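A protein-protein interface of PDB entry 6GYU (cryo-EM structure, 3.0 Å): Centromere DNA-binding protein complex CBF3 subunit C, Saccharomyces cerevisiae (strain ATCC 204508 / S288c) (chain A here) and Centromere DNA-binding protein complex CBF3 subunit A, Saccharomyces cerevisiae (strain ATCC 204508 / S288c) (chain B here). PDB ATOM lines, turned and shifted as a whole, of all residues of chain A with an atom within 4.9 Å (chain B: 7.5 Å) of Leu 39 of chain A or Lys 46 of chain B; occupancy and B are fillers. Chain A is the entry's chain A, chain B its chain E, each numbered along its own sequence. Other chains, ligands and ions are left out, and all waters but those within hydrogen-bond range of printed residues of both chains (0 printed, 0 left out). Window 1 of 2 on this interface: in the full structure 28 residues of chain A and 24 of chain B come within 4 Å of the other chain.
A ring nitrogen (NE2) of His 139 of chain B is in hydrogen-bond range of the backbone carbonyl oxygen of Tyr 40 of chain A, at 2.8 Å.
A ring nitrogen (ND1) of His 43 of chain B lies within hydrogen-bond range of the side-chain hydroxyl (OH) of Tyr 79 of chain A, at 2.4 Å.
The backbone carbonyl oxygen (O) of Leu 39 of chain A lies within hydrogen-bond range of the side-chain hydroxyl (OH) of Tyr 75 of chain B.
The backbone carbonyl oxygen (O) of His 43 of chain B sits at hydrogen-bond distance from the side-chain hydroxyl (OG1) of Thr 47 of chain B.
Among the printed residues, pairs that only touch across the chains: Tyr 40 of chain A with Phe 131 of chain B (3.1 Å), Tyr 79 of chain A with Thr 47 of chain B (3.3 Å), Ser 42 of chain A with Tyr 75 of chain B (3.3 Å), Ile 36 of chain A with His 43 of chain B (3.4 Å), Tyr 79 of chain A with Thr 50 of chain B (3.4 Å), Val 45 of chain A with Tyr 75 of chain B (3.5 Å), Ser 42 of chain A with His 139 of chain B (3.6 Å), Tyr 40 of chain A with Tyr 49 of chain B (3.6 Å), Tyr 79 of chain A with Lys 46 of chain B (3.6 Å), Leu 39 of chain A with Lys 46 of chain B (3.7 Å), Tyr 40 of chain A with Leu 135 of chain B (3.7 Å) and Tyr 34 of chain A with His 43 of chain B (3.8 Å).
Of chain B, only Lys 46 and Tyr 75 come within 4 Å of Leu 39 of chain A.
Of the printed residues of chain A, His 139 of chain B touches Tyr 40 (2.8 Å) and Ser 42 (3.6 Å).
Of the printed residues of chain A, Tyr 75 of chain B touches Leu 39, Ser 42 and Val 45.
Of the printed residues of chain A, His 43 of chain B touches Tyr 34, Ile 36 and Tyr 79.
Of the printed residues of chain B, Tyr 79 of chain A touches His 43, Lys 46, Thr 47 and Thr 50.
The nearest residue of chain B that does not touch Leu 39 of chain A is His 43 of chain B (4.4 Å).
The nearest residue of chain A that does not touch Lys 46 of chain B is Val 45 of chain A (4.3 Å).
The nearest printed residue of chain B that does not touch Tyr 40 of chain A is Ala 42 of chain B (4.2 Å).
Hydrophobic or aromatic side chains of chain A that line the printed part of chain B: Ile 36, Leu 39, Tyr 40, Val 45 and Tyr 79.
Hydrophobic or aromatic side chains of chain B that line the printed part of chain A: His 43, Tyr 49, Tyr 75, Phe 131, Leu 135 and His 139.
Along chain B the printed residues that touch a printed residue of chain A span positions 43 to 139.
Among the printed residues, 15 pairs touch across the chains.
Among the printed residues, no Asp or Glu carboxylate lies within 4 Å of a Lys or Arg side-chain nitrogen of the other chain.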
ATOM      1  N   TYR A  34      17.122  10.908 -28.105  1.00  0.00           N
ATOM      2  CA  TYR A  34      17.324  11.261 -29.502  1.00  0.00           C
ATOM      3  C   TYR A  34      17.575   9.985 -30.289  1.00  0.00           C
ATOM      4  O   TYR A  34      18.270   9.088 -29.797  1.00  0.00           O
ATOM      5  CB  TYR A  34      18.494  12.234 -29.662  1.00  0.00           C
ATOM      6  CG  TYR A  34      18.226  13.628 -29.145  1.00  0.00           C
ATOM      7  CD1 TYR A  34      16.929  14.069 -28.915  1.00  0.00           C
ATOM      8  CD2 TYR A  34      19.272  14.501 -28.881  1.00  0.00           C
ATOM      9  CE1 TYR A  34      16.681  15.342 -28.441  1.00  0.00           C
ATOM     10  CE2 TYR A  34      19.034  15.777 -28.406  1.00  0.00           C
ATOM     11  CZ  TYR A  34      17.738  16.190 -28.188  1.00  0.00           C
ATOM     12  OH  TYR A  34      17.495  17.458 -27.715  1.00  0.00           O
ATOM     13  N   PRO A  35      16.998   9.846 -31.482  1.00  0.00           N
ATOM     14  CA  PRO A  35      17.287   8.669 -32.303  1.00  0.00           C
ATOM     15  C   PRO A  35      18.726   8.706 -32.771  1.00  0.00           C
ATOM     16  O   PRO A  35      19.314   9.775 -32.950  1.00  0.00           O
ATOM     17  CB  PRO A  35      16.311   8.804 -33.475  1.00  0.00           C
ATOM     18  CG  PRO A  35      16.057  10.261 -33.569  1.00  0.00           C
ATOM     19  CD  PRO A  35      16.097  10.787 -32.165  1.00  0.00           C
ATOM     20  N   ILE A  36      19.307   7.525 -32.965  1.00  0.00           N
ATOM     21  CA  ILE A  36      20.753   7.488 -33.125  1.00  0.00           C
ATOM     22  C   ILE A  36      21.045   7.698 -34.604  1.00  0.00           C
ATOM     23  O   ILE A  36      21.436   6.769 -35.317  1.00  0.00           O
ATOM     24  CB  ILE A  36      21.349   6.154 -32.630  1.00  0.00           C
ATOM     25  CG1 ILE A  36      20.761   5.731 -31.284  1.00  0.00           C
ATOM     26  CG2 ILE A  36      22.821   6.293 -32.402  1.00  0.00           C
ATOM     27  CD1 ILE A  36      19.671   4.657 -31.381  1.00  0.00           C
ATOM     28  N   ASP A  37      20.837   8.923 -35.073  1.00  0.00           N
ATOM     29  CA  ASP A  37      21.363   9.393 -36.342  1.00  0.00           C
ATOM     30  C   ASP A  37      21.753  10.850 -36.165  1.00  0.00           C
ATOM     31  O   ASP A  37      22.644  11.355 -36.848  1.00  0.00           O
ATOM     32  CB  ASP A  37      20.332   9.220 -37.457  1.00  0.00           C
ATOM     33  CG  ASP A  37      20.890   9.553 -38.824  1.00  0.00           C
ATOM     34  OD1 ASP A  37      21.674   8.744 -39.361  1.00  0.00           O
ATOM     35  OD2 ASP A  37      20.546  10.627 -39.361  1.00  0.00           O
ATOM     36  N   ILE A  38      21.087  11.517 -35.225  1.00  0.00           N
ATOM     37  CA  ILE A  38      21.359  12.917 -34.927  1.00  0.00           C
ATOM     38  C   ILE A  38      22.537  13.036 -33.965  1.00  0.00           C
ATOM     39  O   ILE A  38      23.361  13.949 -34.102  1.00  0.00           O
ATOM     40  CB  ILE A  38      20.081  13.599 -34.382  1.00  0.00           C
ATOM     41  CG1 ILE A  38      19.037  13.784 -35.491  1.00  0.00           C
ATOM     42  CG2 ILE A  38      20.356  14.954 -33.734  1.00  0.00           C
ATOM     43  CD1 ILE A  38      17.996  12.693 -35.595  1.00  0.00           C
ATOM     44  N   LEU A  39      22.676  12.076 -33.046  1.00  0.00           N
ATOM     45  CA  LEU A  39      23.802  12.055 -32.121  1.00  0.00           C
ATOM     46  C   LEU A  39      25.128  11.815 -32.835  1.00  0.00           C
ATOM     47  O   LEU A  39      26.185  12.167 -32.301  1.00  0.00           O
ATOM     48  CB  LEU A  39      23.580  10.975 -31.066  1.00  0.00           C
ATOM     49  CG  LEU A  39      22.373  11.175 -30.154  1.00  0.00           C
ATOM     50  CD1 LEU A  39      22.154   9.950 -29.288  1.00  0.00           C
ATOM     51  CD2 LEU A  39      22.554  12.416 -29.303  1.00  0.00           C
ATOM     52  N   TYR A  40      25.099  11.229 -34.030  1.00  0.00           N
ATOM     53  CA  TYR A  40      26.321  10.954 -34.773  1.00  0.00           C
ATOM     54  C   TYR A  40      26.534  11.922 -35.928  1.00  0.00           C
ATOM     55  O   TYR A  40      27.677  12.170 -36.314  1.00  0.00           O
ATOM     56  CB  TYR A  40      26.324   9.517 -35.311  1.00  0.00           C
ATOM     57  CG  TYR A  40      26.346   8.416 -34.263  1.00  0.00           C
ATOM     58  CD1 TYR A  40      26.625   8.686 -32.926  1.00  0.00           C
ATOM     59  CD2 TYR A  40      26.099   7.098 -34.623  1.00  0.00           C
ATOM     60  CE1 TYR A  40      26.632   7.683 -31.981  1.00  0.00           C
ATOM     61  CE2 TYR A  40      26.122   6.085 -33.685  1.00  0.00           C
ATOM     62  CZ  TYR A  40      26.382   6.387 -32.366  1.00  0.00           C
ATOM     63  OH  TYR A  40      26.395   5.392 -31.421  1.00  0.00           O
ATOM     64  N   LYS A  41      25.459  12.481 -36.494  1.00  0.00           N
ATOM     65  CA  LYS A  41      25.570  13.521 -37.522  1.00  0.00           C
ATOM     66  C   LYS A  41      25.524  14.897 -36.858  1.00  0.00           C
ATOM     67  O   LYS A  41      24.727  15.773 -37.201  1.00  0.00           O
ATOM     68  CB  LYS A  41      24.468  13.391 -38.563  1.00  0.00           C
ATOM     69  CG  LYS A  41      24.546  12.154 -39.426  1.00  0.00           C
ATOM     70  CD  LYS A  41      23.432  12.133 -40.456  1.00  0.00           C
ATOM     71  CE  LYS A  41      23.606  10.986 -41.439  1.00  0.00           C
ATOM     72  NZ  LYS A  41      23.451   9.656 -40.796  1.00  0.00           N
ATOM     73  N   SER A  42      26.405  15.078 -35.881  1.00  0.00           N
ATOM     74  CA  SER A  42      26.517  16.345 -35.183  1.00  0.00           C
ATOM     75  C   SER A  42      27.965  16.535 -34.769  1.00  0.00           C
ATOM     76  O   SER A  42      28.667  15.569 -34.460  1.00  0.00           O
ATOM     77  CB  SER A  42      25.600  16.404 -33.958  1.00  0.00           C
ATOM     78  N   VAL A  45      28.961  17.084 -28.760  1.00  0.00           N
ATOM     79  CA  VAL A  45      28.548  15.928 -27.971  1.00  0.00           C
ATOM     80  C   VAL A  45      27.843  16.456 -26.732  1.00  0.00           C
ATOM     81  O   VAL A  45      28.492  17.018 -25.842  1.00  0.00           O
ATOM     82  CB  VAL A  45      29.739  15.046 -27.570  1.00  0.00           C
ATOM     83  CG1 VAL A  45      29.270  13.876 -26.723  1.00  0.00           C
ATOM     84  CG2 VAL A  45      30.491  14.565 -28.786  1.00  0.00           C
ATOM     85  N   GLU A  46      26.525  16.274 -26.670  1.00  0.00           N
ATOM     86  CA  GLU A  46      25.737  16.820 -25.569  1.00  0.00           C
ATOM     87  C   GLU A  46      26.058  16.090 -24.271  1.00  0.00           C
ATOM     88  O   GLU A  46      25.970  14.859 -24.199  1.00  0.00           O
ATOM     89  CB  GLU A  46      24.248  16.725 -25.884  1.00  0.00           C
ATOM     90  CG  GLU A  46      23.797  17.638 -27.010  1.00  0.00           C
ATOM     91  CD  GLU A  46      22.312  17.526 -27.289  1.00  0.00           C
ATOM     92  OE1 GLU A  46      21.658  16.653 -26.681  1.00  0.00           O
ATOM     93  OE2 GLU A  46      21.798  18.307 -28.116  1.00  0.00           O
ATOM     94  N   TYR A  79      23.681   8.929 -19.518  1.00  0.00           N
ATOM     95  CA  TYR A  79      24.013  10.165 -20.203  1.00  0.00           C
ATOM     96  C   TYR A  79      22.761  11.030 -20.257  1.00  0.00           C
ATOM     97  O   TYR A  79      21.667  10.536 -20.548  1.00  0.00           O
ATOM     98  CB  TYR A  79      24.555   9.881 -21.611  1.00  0.00           C
ATOM     99  CG  TYR A  79      23.546   9.336 -22.598  1.00  0.00           C
ATOM    100  CD1 TYR A  79      23.247   7.983 -22.642  1.00  0.00           C
ATOM    101  CD2 TYR A  79      22.906  10.179 -23.501  1.00  0.00           C
ATOM    102  CE1 TYR A  79      22.323   7.490 -23.539  1.00  0.00           C
ATOM    103  CE2 TYR A  79      21.984   9.695 -24.396  1.00  0.00           C
ATOM    104  CZ  TYR A  79      21.700   8.352 -24.413  1.00  0.00           C
ATOM    105  OH  TYR A  79      20.783   7.875 -25.311  1.00  0.00           O
ATOM    106  N   LEU B  37      25.289  -1.719 -34.524  1.00  0.00           N
ATOM    107  CA  LEU B  37      24.960  -1.938 -33.124  1.00  0.00           C
ATOM    108  C   LEU B  37      23.454  -2.009 -32.939  1.00  0.00           C
ATOM    109  O   LEU B  37      22.685  -1.446 -33.721  1.00  0.00           O
ATOM    110  CB  LEU B  37      25.504  -0.826 -32.229  1.00  0.00           C
ATOM    111  CG  LEU B  37      27.010  -0.683 -32.069  1.00  0.00           C
ATOM    112  CD1 LEU B  37      27.290   0.555 -31.257  1.00  0.00           C
ATOM    113  CD2 LEU B  37      27.588  -1.909 -31.395  1.00  0.00           C
ATOM    114  N   ARG B  40      20.031  -0.579 -27.925  1.00  0.00           N
ATOM    115  CA  ARG B  40      20.395  -0.745 -26.521  1.00  0.00           C
ATOM    116  C   ARG B  40      21.904  -0.698 -26.335  1.00  0.00           C
ATOM    117  O   ARG B  40      22.405  -0.011 -25.437  1.00  0.00           O
ATOM    118  CB  ARG B  40      19.842  -2.070 -26.000  1.00  0.00           C
ATOM    119  CG  ARG B  40      20.032  -2.296 -24.518  1.00  0.00           C
ATOM    120  CD  ARG B  40      19.498  -3.659 -24.121  1.00  0.00           C
ATOM    121  NE  ARG B  40      19.670  -3.925 -22.698  1.00  0.00           N
ATOM    122  CZ  ARG B  40      18.751  -3.660 -21.776  1.00  0.00           C
ATOM    123  NH1 ARG B  40      17.587  -3.139 -22.132  1.00  0.00           N
ATOM    124  NH2 ARG B  40      18.989  -3.932 -20.500  1.00  0.00           N
ATOM    125  N   THR B  41      22.641  -1.405 -27.196  1.00  0.00           N
ATOM    126  CA  THR B  41      24.097  -1.388 -27.145  1.00  0.00           C
ATOM    127  C   THR B  41      24.648  -0.012 -27.501  1.00  0.00           C
ATOM    128  O   THR B  41      25.632   0.431 -26.900  1.00  0.00           O
ATOM    129  CB  THR B  41      24.648  -2.460 -28.087  1.00  0.00           C
ATOM    130  OG1 THR B  41      24.061  -3.723 -27.757  1.00  0.00           O
ATOM    131  CG2 THR B  41      26.151  -2.593 -27.950  1.00  0.00           C
ATOM    132  N   ALA B  42      23.992   0.695 -28.426  1.00  0.00           N
ATOM    133  CA  ALA B  42      24.440   2.033 -28.805  1.00  0.00           C
ATOM    134  C   ALA B  42      24.274   3.025 -27.662  1.00  0.00           C
ATOM    135  O   ALA B  42      25.180   3.819 -27.388  1.00  0.00           O
ATOM    136  CB  ALA B  42      23.684   2.516 -30.039  1.00  0.00           C
ATOM    137  N   HIS B  43      23.147   2.972 -26.954  1.00  0.00           N
ATOM    138  CA  HIS B  43      22.992   3.900 -25.841  1.00  0.00           C
ATOM    139  C   HIS B  43      23.801   3.483 -24.614  1.00  0.00           C
ATOM    140  O   HIS B  43      24.223   4.356 -23.846  1.00  0.00           O
ATOM    141  CB  HIS B  43      21.518   4.072 -25.478  1.00  0.00           C
ATOM    142  CG  HIS B  43      20.692   4.726 -26.544  1.00  0.00           C
ATOM    143  ND1 HIS B  43      20.859   6.041 -26.915  1.00  0.00           N
ATOM    144  CD2 HIS B  43      19.644   4.263 -27.264  1.00  0.00           C
ATOM    145  CE1 HIS B  43      19.982   6.346 -27.854  1.00  0.00           C
ATOM    146  NE2 HIS B  43      19.229   5.287 -28.080  1.00  0.00           N
ATOM    147  N   GLN B  44      24.058   2.179 -24.415  1.00  0.00           N
ATOM    148  CA  GLN B  44      25.001   1.765 -23.371  1.00  0.00           C
ATOM    149  C   GLN B  44      26.406   2.269 -23.661  1.00  0.00           C
ATOM    150  O   GLN B  44      27.109   2.744 -22.753  1.00  0.00           O
ATOM    151  CB  GLN B  44      25.035   0.244 -23.229  1.00  0.00           C
ATOM    152  CG  GLN B  44      23.875  -0.373 -22.490  1.00  0.00           C
ATOM    153  CD  GLN B  44      24.010  -1.877 -22.375  1.00  0.00           C
ATOM    154  OE1 GLN B  44      24.932  -2.472 -22.932  1.00  0.00           O
ATOM    155  NE2 GLN B  44      23.097  -2.500 -21.641  1.00  0.00           N
ATOM    156  N   TYR B  45      26.836   2.173 -24.922  1.00  0.00           N
ATOM    157  CA  TYR B  45      28.148   2.679 -25.293  1.00  0.00           C
ATOM    158  C   TYR B  45      28.211   4.189 -25.146  1.00  0.00           C
ATOM    159  O   TYR B  45      29.238   4.725 -24.720  1.00  0.00           O
ATOM    160  CB  TYR B  45      28.510   2.266 -26.719  1.00  0.00           C
ATOM    161  CG  TYR B  45      28.865   0.805 -26.900  1.00  0.00           C
ATOM    162  CD1 TYR B  45      29.000  -0.049 -25.812  1.00  0.00           C
ATOM    163  CD2 TYR B  45      29.118   0.294 -28.163  1.00  0.00           C
ATOM    164  CE1 TYR B  45      29.336  -1.375 -25.982  1.00  0.00           C
ATOM    165  CE2 TYR B  45      29.459  -1.030 -28.343  1.00  0.00           C
ATOM    166  CZ  TYR B  45      29.568  -1.859 -27.249  1.00  0.00           C
ATOM    167  OH  TYR B  45      29.906  -3.179 -27.422  1.00  0.00           O
ATOM    168  N   LYS B  46      27.111   4.885 -25.456  1.00  0.00           N
ATOM    169  CA  LYS B  46      27.091   6.334 -25.284  1.00  0.00           C
ATOM    170  C   LYS B  46      27.132   6.722 -23.812  1.00  0.00           C
ATOM    171  O   LYS B  46      27.769   7.720 -23.464  1.00  0.00           O
ATOM    172  CB  LYS B  46      25.864   6.941 -25.963  1.00  0.00           C
ATOM    173  CG  LYS B  46      25.874   8.461 -25.966  1.00  0.00           C
ATOM    174  CD  LYS B  46      24.740   9.055 -26.753  1.00  0.00           C
ATOM    175  CE  LYS B  46      24.748  10.565 -26.625  1.00  0.00           C
ATOM    176  NZ  LYS B  46      25.960  11.158 -27.250  1.00  0.00           N
ATOM    177  N   THR B  47      26.509   5.924 -22.942  1.00  0.00           N
ATOM    178  CA  THR B  47      26.633   6.125 -21.499  1.00  0.00           C
ATOM    179  C   THR B  47      28.082   5.982 -21.045  1.00  0.00           C
ATOM    180  O   THR B  47      28.598   6.814 -20.284  1.00  0.00           O
ATOM    181  CB  THR B  47      25.744   5.122 -20.765  1.00  0.00           C
ATOM    182  OG1 THR B  47      24.378   5.334 -21.135  1.00  0.00           O
ATOM    183  CG2 THR B  47      25.885   5.267 -19.267  1.00  0.00           C
ATOM    184  N   TYR B  48      28.770   4.958 -21.551  1.00  0.00           N
ATOM    185  CA  TYR B  48      30.146   4.710 -21.124  1.00  0.00           C
ATOM    186  C   TYR B  48      31.112   5.772 -21.647  1.00  0.00           C
ATOM    187  O   TYR B  48      31.959   6.271 -20.890  1.00  0.00           O
ATOM    188  CB  TYR B  48      30.570   3.313 -21.559  1.00  0.00           C
ATOM    189  CG  TYR B  48      29.898   2.212 -20.774  1.00  0.00           C
ATOM    190  CD1 TYR B  48      29.358   2.456 -19.517  1.00  0.00           C
ATOM    191  CD2 TYR B  48      29.773   0.936 -21.301  1.00  0.00           C
ATOM    192  CE1 TYR B  48      28.735   1.456 -18.800  1.00  0.00           C
ATOM    193  CE2 TYR B  48      29.148  -0.068 -20.592  1.00  0.00           C
ATOM    194  CZ  TYR B  48      28.632   0.197 -19.344  1.00  0.00           C
ATOM    195  OH  TYR B  48      28.011  -0.806 -18.637  1.00  0.00           O
ATOM    196  N   TYR B  49      30.996   6.171 -22.917  1.00  0.00           N
ATOM    197  CA  TYR B  49      31.903   7.242 -23.318  1.00  0.00           C
ATOM    198  C   TYR B  49      31.449   8.614 -22.837  1.00  0.00           C
ATOM    199  O   TYR B  49      32.263   9.537 -22.831  1.00  0.00           O
ATOM    200  CB  TYR B  49      32.196   7.283 -24.836  1.00  0.00           C
ATOM    201  CG  TYR B  49      31.103   7.541 -25.866  1.00  0.00           C
ATOM    202  CD1 TYR B  49      30.682   6.531 -26.717  1.00  0.00           C
ATOM    203  CD2 TYR B  49      30.533   8.801 -26.025  1.00  0.00           C
ATOM    204  CE1 TYR B  49      29.711   6.752 -27.673  1.00  0.00           C
ATOM    205  CE2 TYR B  49      29.553   9.030 -26.973  1.00  0.00           C
ATOM    206  CZ  TYR B  49      29.147   8.002 -27.792  1.00  0.00           C
ATOM    207  OH  TYR B  49      28.176   8.229 -28.737  1.00  0.00           O
ATOM    208  N   THR B  50      30.207   8.768 -22.379  1.00  0.00           N
ATOM    209  CA  THR B  50      29.848   9.993 -21.681  1.00  0.00           C
ATOM    210  C   THR B  50      30.520  10.054 -20.317  1.00  0.00           C
ATOM    211  O   THR B  50      30.971  11.127 -19.903  1.00  0.00           O
ATOM    212  CB  THR B  50      28.328  10.092 -21.558  1.00  0.00           C
ATOM    213  OG1 THR B  50      27.750  10.019 -22.866  1.00  0.00           O
ATOM    214  CG2 THR B  50      27.913  11.409 -20.929  1.00  0.00           C
ATOM    215  N   LYS B  51      30.621   8.907 -19.627  1.00  0.00           N
ATOM    216  CA  LYS B  51      31.464   8.814 -18.433  1.00  0.00           C
ATOM    217  C   LYS B  51      32.913   9.175 -18.743  1.00  0.00           C
ATOM    218  O   LYS B  51      33.563   9.890 -17.968  1.00  0.00           O
ATOM    219  CB  LYS B  51      31.403   7.406 -17.839  1.00  0.00           C
ATOM    220  CG  LYS B  51      30.051   6.964 -17.322  1.00  0.00           C
ATOM    221  CD  LYS B  51      29.684   7.669 -16.035  1.00  0.00           C
ATOM    222  CE  LYS B  51      28.335   7.192 -15.529  1.00  0.00           C
ATOM    223  NZ  LYS B  51      28.389   5.767 -15.100  1.00  0.00           N
ATOM    224  N   TYR B  52      33.417   8.713 -19.893  1.00  0.00           N
ATOM    225  CA  TYR B  52      34.787   9.030 -20.304  1.00  0.00           C
ATOM    226  C   TYR B  52      34.988  10.521 -20.564  1.00  0.00           C
ATOM    227  O   TYR B  52      35.999  11.096 -20.144  1.00  0.00           O
ATOM    228  CB  TYR B  52      35.159   8.228 -21.545  1.00  0.00           C
ATOM    229  CG  TYR B  52      36.520   8.564 -22.104  1.00  0.00           C
ATOM    230  CD1 TYR B  52      37.678   8.145 -21.464  1.00  0.00           C
ATOM    231  CD2 TYR B  52      36.647   9.297 -23.277  1.00  0.00           C
ATOM    232  CE1 TYR B  52      38.923   8.452 -21.974  1.00  0.00           C
ATOM    233  CE2 TYR B  52      37.886   9.608 -23.792  1.00  0.00           C
ATOM    234  CZ  TYR B  52      39.019   9.183 -23.138  1.00  0.00           C
ATOM    235  OH  TYR B  52      40.255   9.492 -23.652  1.00  0.00           O
ATOM    236  N   ILE B  53      34.046  11.165 -21.251  1.00  0.00           N
ATOM    237  CA  ILE B  53      34.216  12.575 -21.588  1.00  0.00           C
ATOM    238  C   ILE B  53      34.000  13.455 -20.356  1.00  0.00           C
ATOM    239  O   ILE B  53      34.669  14.485 -20.190  1.00  0.00           O
ATOM    240  CB  ILE B  53      33.290  12.950 -22.762  1.00  0.00           C
ATOM    241  CG1 ILE B  53      33.692  12.171 -24.011  1.00  0.00           C
ATOM    242  CG2 ILE B  53      33.413  14.398 -23.121  1.00  0.00           C
ATOM    243  CD1 ILE B  53      32.680  12.240 -25.127  1.00  0.00           C
ATOM    244  N   TYR B  75      33.596  16.177 -31.842  1.00  0.00           N
ATOM    245  CA  TYR B  75      34.284  14.931 -32.160  1.00  0.00           C
ATOM    246  C   TYR B  75      35.632  15.173 -32.822  1.00  0.00           C
ATOM    247  O   TYR B  75      36.490  14.285 -32.796  1.00  0.00           O
ATOM    248  CB  TYR B  75      33.436  14.060 -33.084  1.00  0.00           C
ATOM    249  CG  TYR B  75      32.193  13.459 -32.476  1.00  0.00           C
ATOM    250  CD1 TYR B  75      32.271  12.346 -31.649  1.00  0.00           C
ATOM    251  CD2 TYR B  75      30.938  13.973 -32.767  1.00  0.00           C
ATOM    252  CE1 TYR B  75      31.134  11.782 -31.103  1.00  0.00           C
ATOM    253  CE2 TYR B  75      29.795  13.416 -32.228  1.00  0.00           C
ATOM    254  CZ  TYR B  75      29.900  12.318 -31.401  1.00  0.00           C
ATOM    255  OH  TYR B  75      28.765  11.763 -30.860  1.00  0.00           O
ATOM    256  N   SER B 128      33.133   0.210 -25.834  1.00  0.00           N
ATOM    257  CA  SER B 128      32.495   1.500 -26.079  1.00  0.00           C
ATOM    258  C   SER B 128      33.506   2.552 -26.501  1.00  0.00           C
ATOM    259  O   SER B 128      33.228   3.372 -27.378  1.00  0.00           O
ATOM    260  CB  SER B 128      31.771   1.973 -24.828  1.00  0.00           C
ATOM    261  OG  SER B 128      32.709   2.338 -23.838  1.00  0.00           O
ATOM    262  N   PHE B 131      34.502   1.911 -29.958  1.00  0.00           N
ATOM    263  CA  PHE B 131      33.474   2.448 -30.843  1.00  0.00           C
ATOM    264  C   PHE B 131      33.551   3.968 -30.934  1.00  0.00           C
ATOM    265  O   PHE B 131      33.287   4.540 -31.992  1.00  0.00           O
ATOM    266  CB  PHE B 131      32.090   2.017 -30.370  1.00  0.00           C
ATOM    267  CG  PHE B 131      30.986   2.473 -31.269  1.00  0.00           C
ATOM    268  CD1 PHE B 131      30.752   1.829 -32.471  1.00  0.00           C
ATOM    269  CD2 PHE B 131      30.192   3.553 -30.924  1.00  0.00           C
ATOM    270  CE1 PHE B 131      29.744   2.250 -33.308  1.00  0.00           C
ATOM    271  CE2 PHE B 131      29.190   3.979 -31.758  1.00  0.00           C
ATOM    272  CZ  PHE B 131      28.961   3.326 -32.951  1.00  0.00           C
ATOM    273  N   LEU B 132      33.909   4.636 -29.838  1.00  0.00           N
ATOM    274  CA  LEU B 132      34.064   6.088 -29.871  1.00  0.00           C
ATOM    275  C   LEU B 132      35.269   6.503 -30.704  1.00  0.00           C
ATOM    276  O   LEU B 132      35.199   7.493 -31.442  1.00  0.00           O
ATOM    277  CB  LEU B 132      34.198   6.645 -28.456  1.00  0.00           C
ATOM    278  CG  LEU B 132      34.286   8.172 -28.385  1.00  0.00           C
ATOM    279  CD1 LEU B 132      32.973   8.810 -28.804  1.00  0.00           C
ATOM    280  CD2 LEU B 132      34.746   8.665 -27.026  1.00  0.00           C
ATOM    281  N   LEU B 135      34.156   6.226 -34.103  1.00  0.00           N
ATOM    282  CA  LEU B 135      33.221   7.310 -34.380  1.00  0.00           C
ATOM    283  C   LEU B 135      33.909   8.655 -34.577  1.00  0.00           C
ATOM    284  O   LEU B 135      33.371   9.524 -35.272  1.00  0.00           O
ATOM    285  CB  LEU B 135      32.202   7.403 -33.236  1.00  0.00           C
ATOM    286  CG  LEU B 135      31.129   8.493 -33.135  1.00  0.00           C
ATOM    287  CD1 LEU B 135      30.210   8.504 -34.333  1.00  0.00           C
ATOM    288  CD2 LEU B 135      30.326   8.305 -31.860  1.00  0.00           C
ATOM    289  N   HIS B 139      34.663  11.764 -38.228  1.00  0.00           N
ATOM    290  CA  HIS B 139      34.584  13.202 -38.011  1.00  0.00           C
ATOM    291  C   HIS B 139      35.938  13.896 -38.091  1.00  0.00           C
ATOM    292  O   HIS B 139      36.043  15.044 -37.648  1.00  0.00           O
ATOM    293  CB  HIS B 139      33.945  13.504 -36.657  1.00  0.00           C
ATOM    294  CG  HIS B 139      32.473  13.246 -36.609  1.00  0.00           C
ATOM    295  ND1 HIS B 139      31.552  14.118 -37.146  1.00  0.00           N
ATOM    296  CD2 HIS B 139      31.762  12.217 -36.093  1.00  0.00           C
ATOM    297  CE1 HIS B 139      30.336  13.640 -36.960  1.00  0.00           C
ATOM    298  NE2 HIS B 139      30.435  12.486 -36.325  1.00  0.00           N
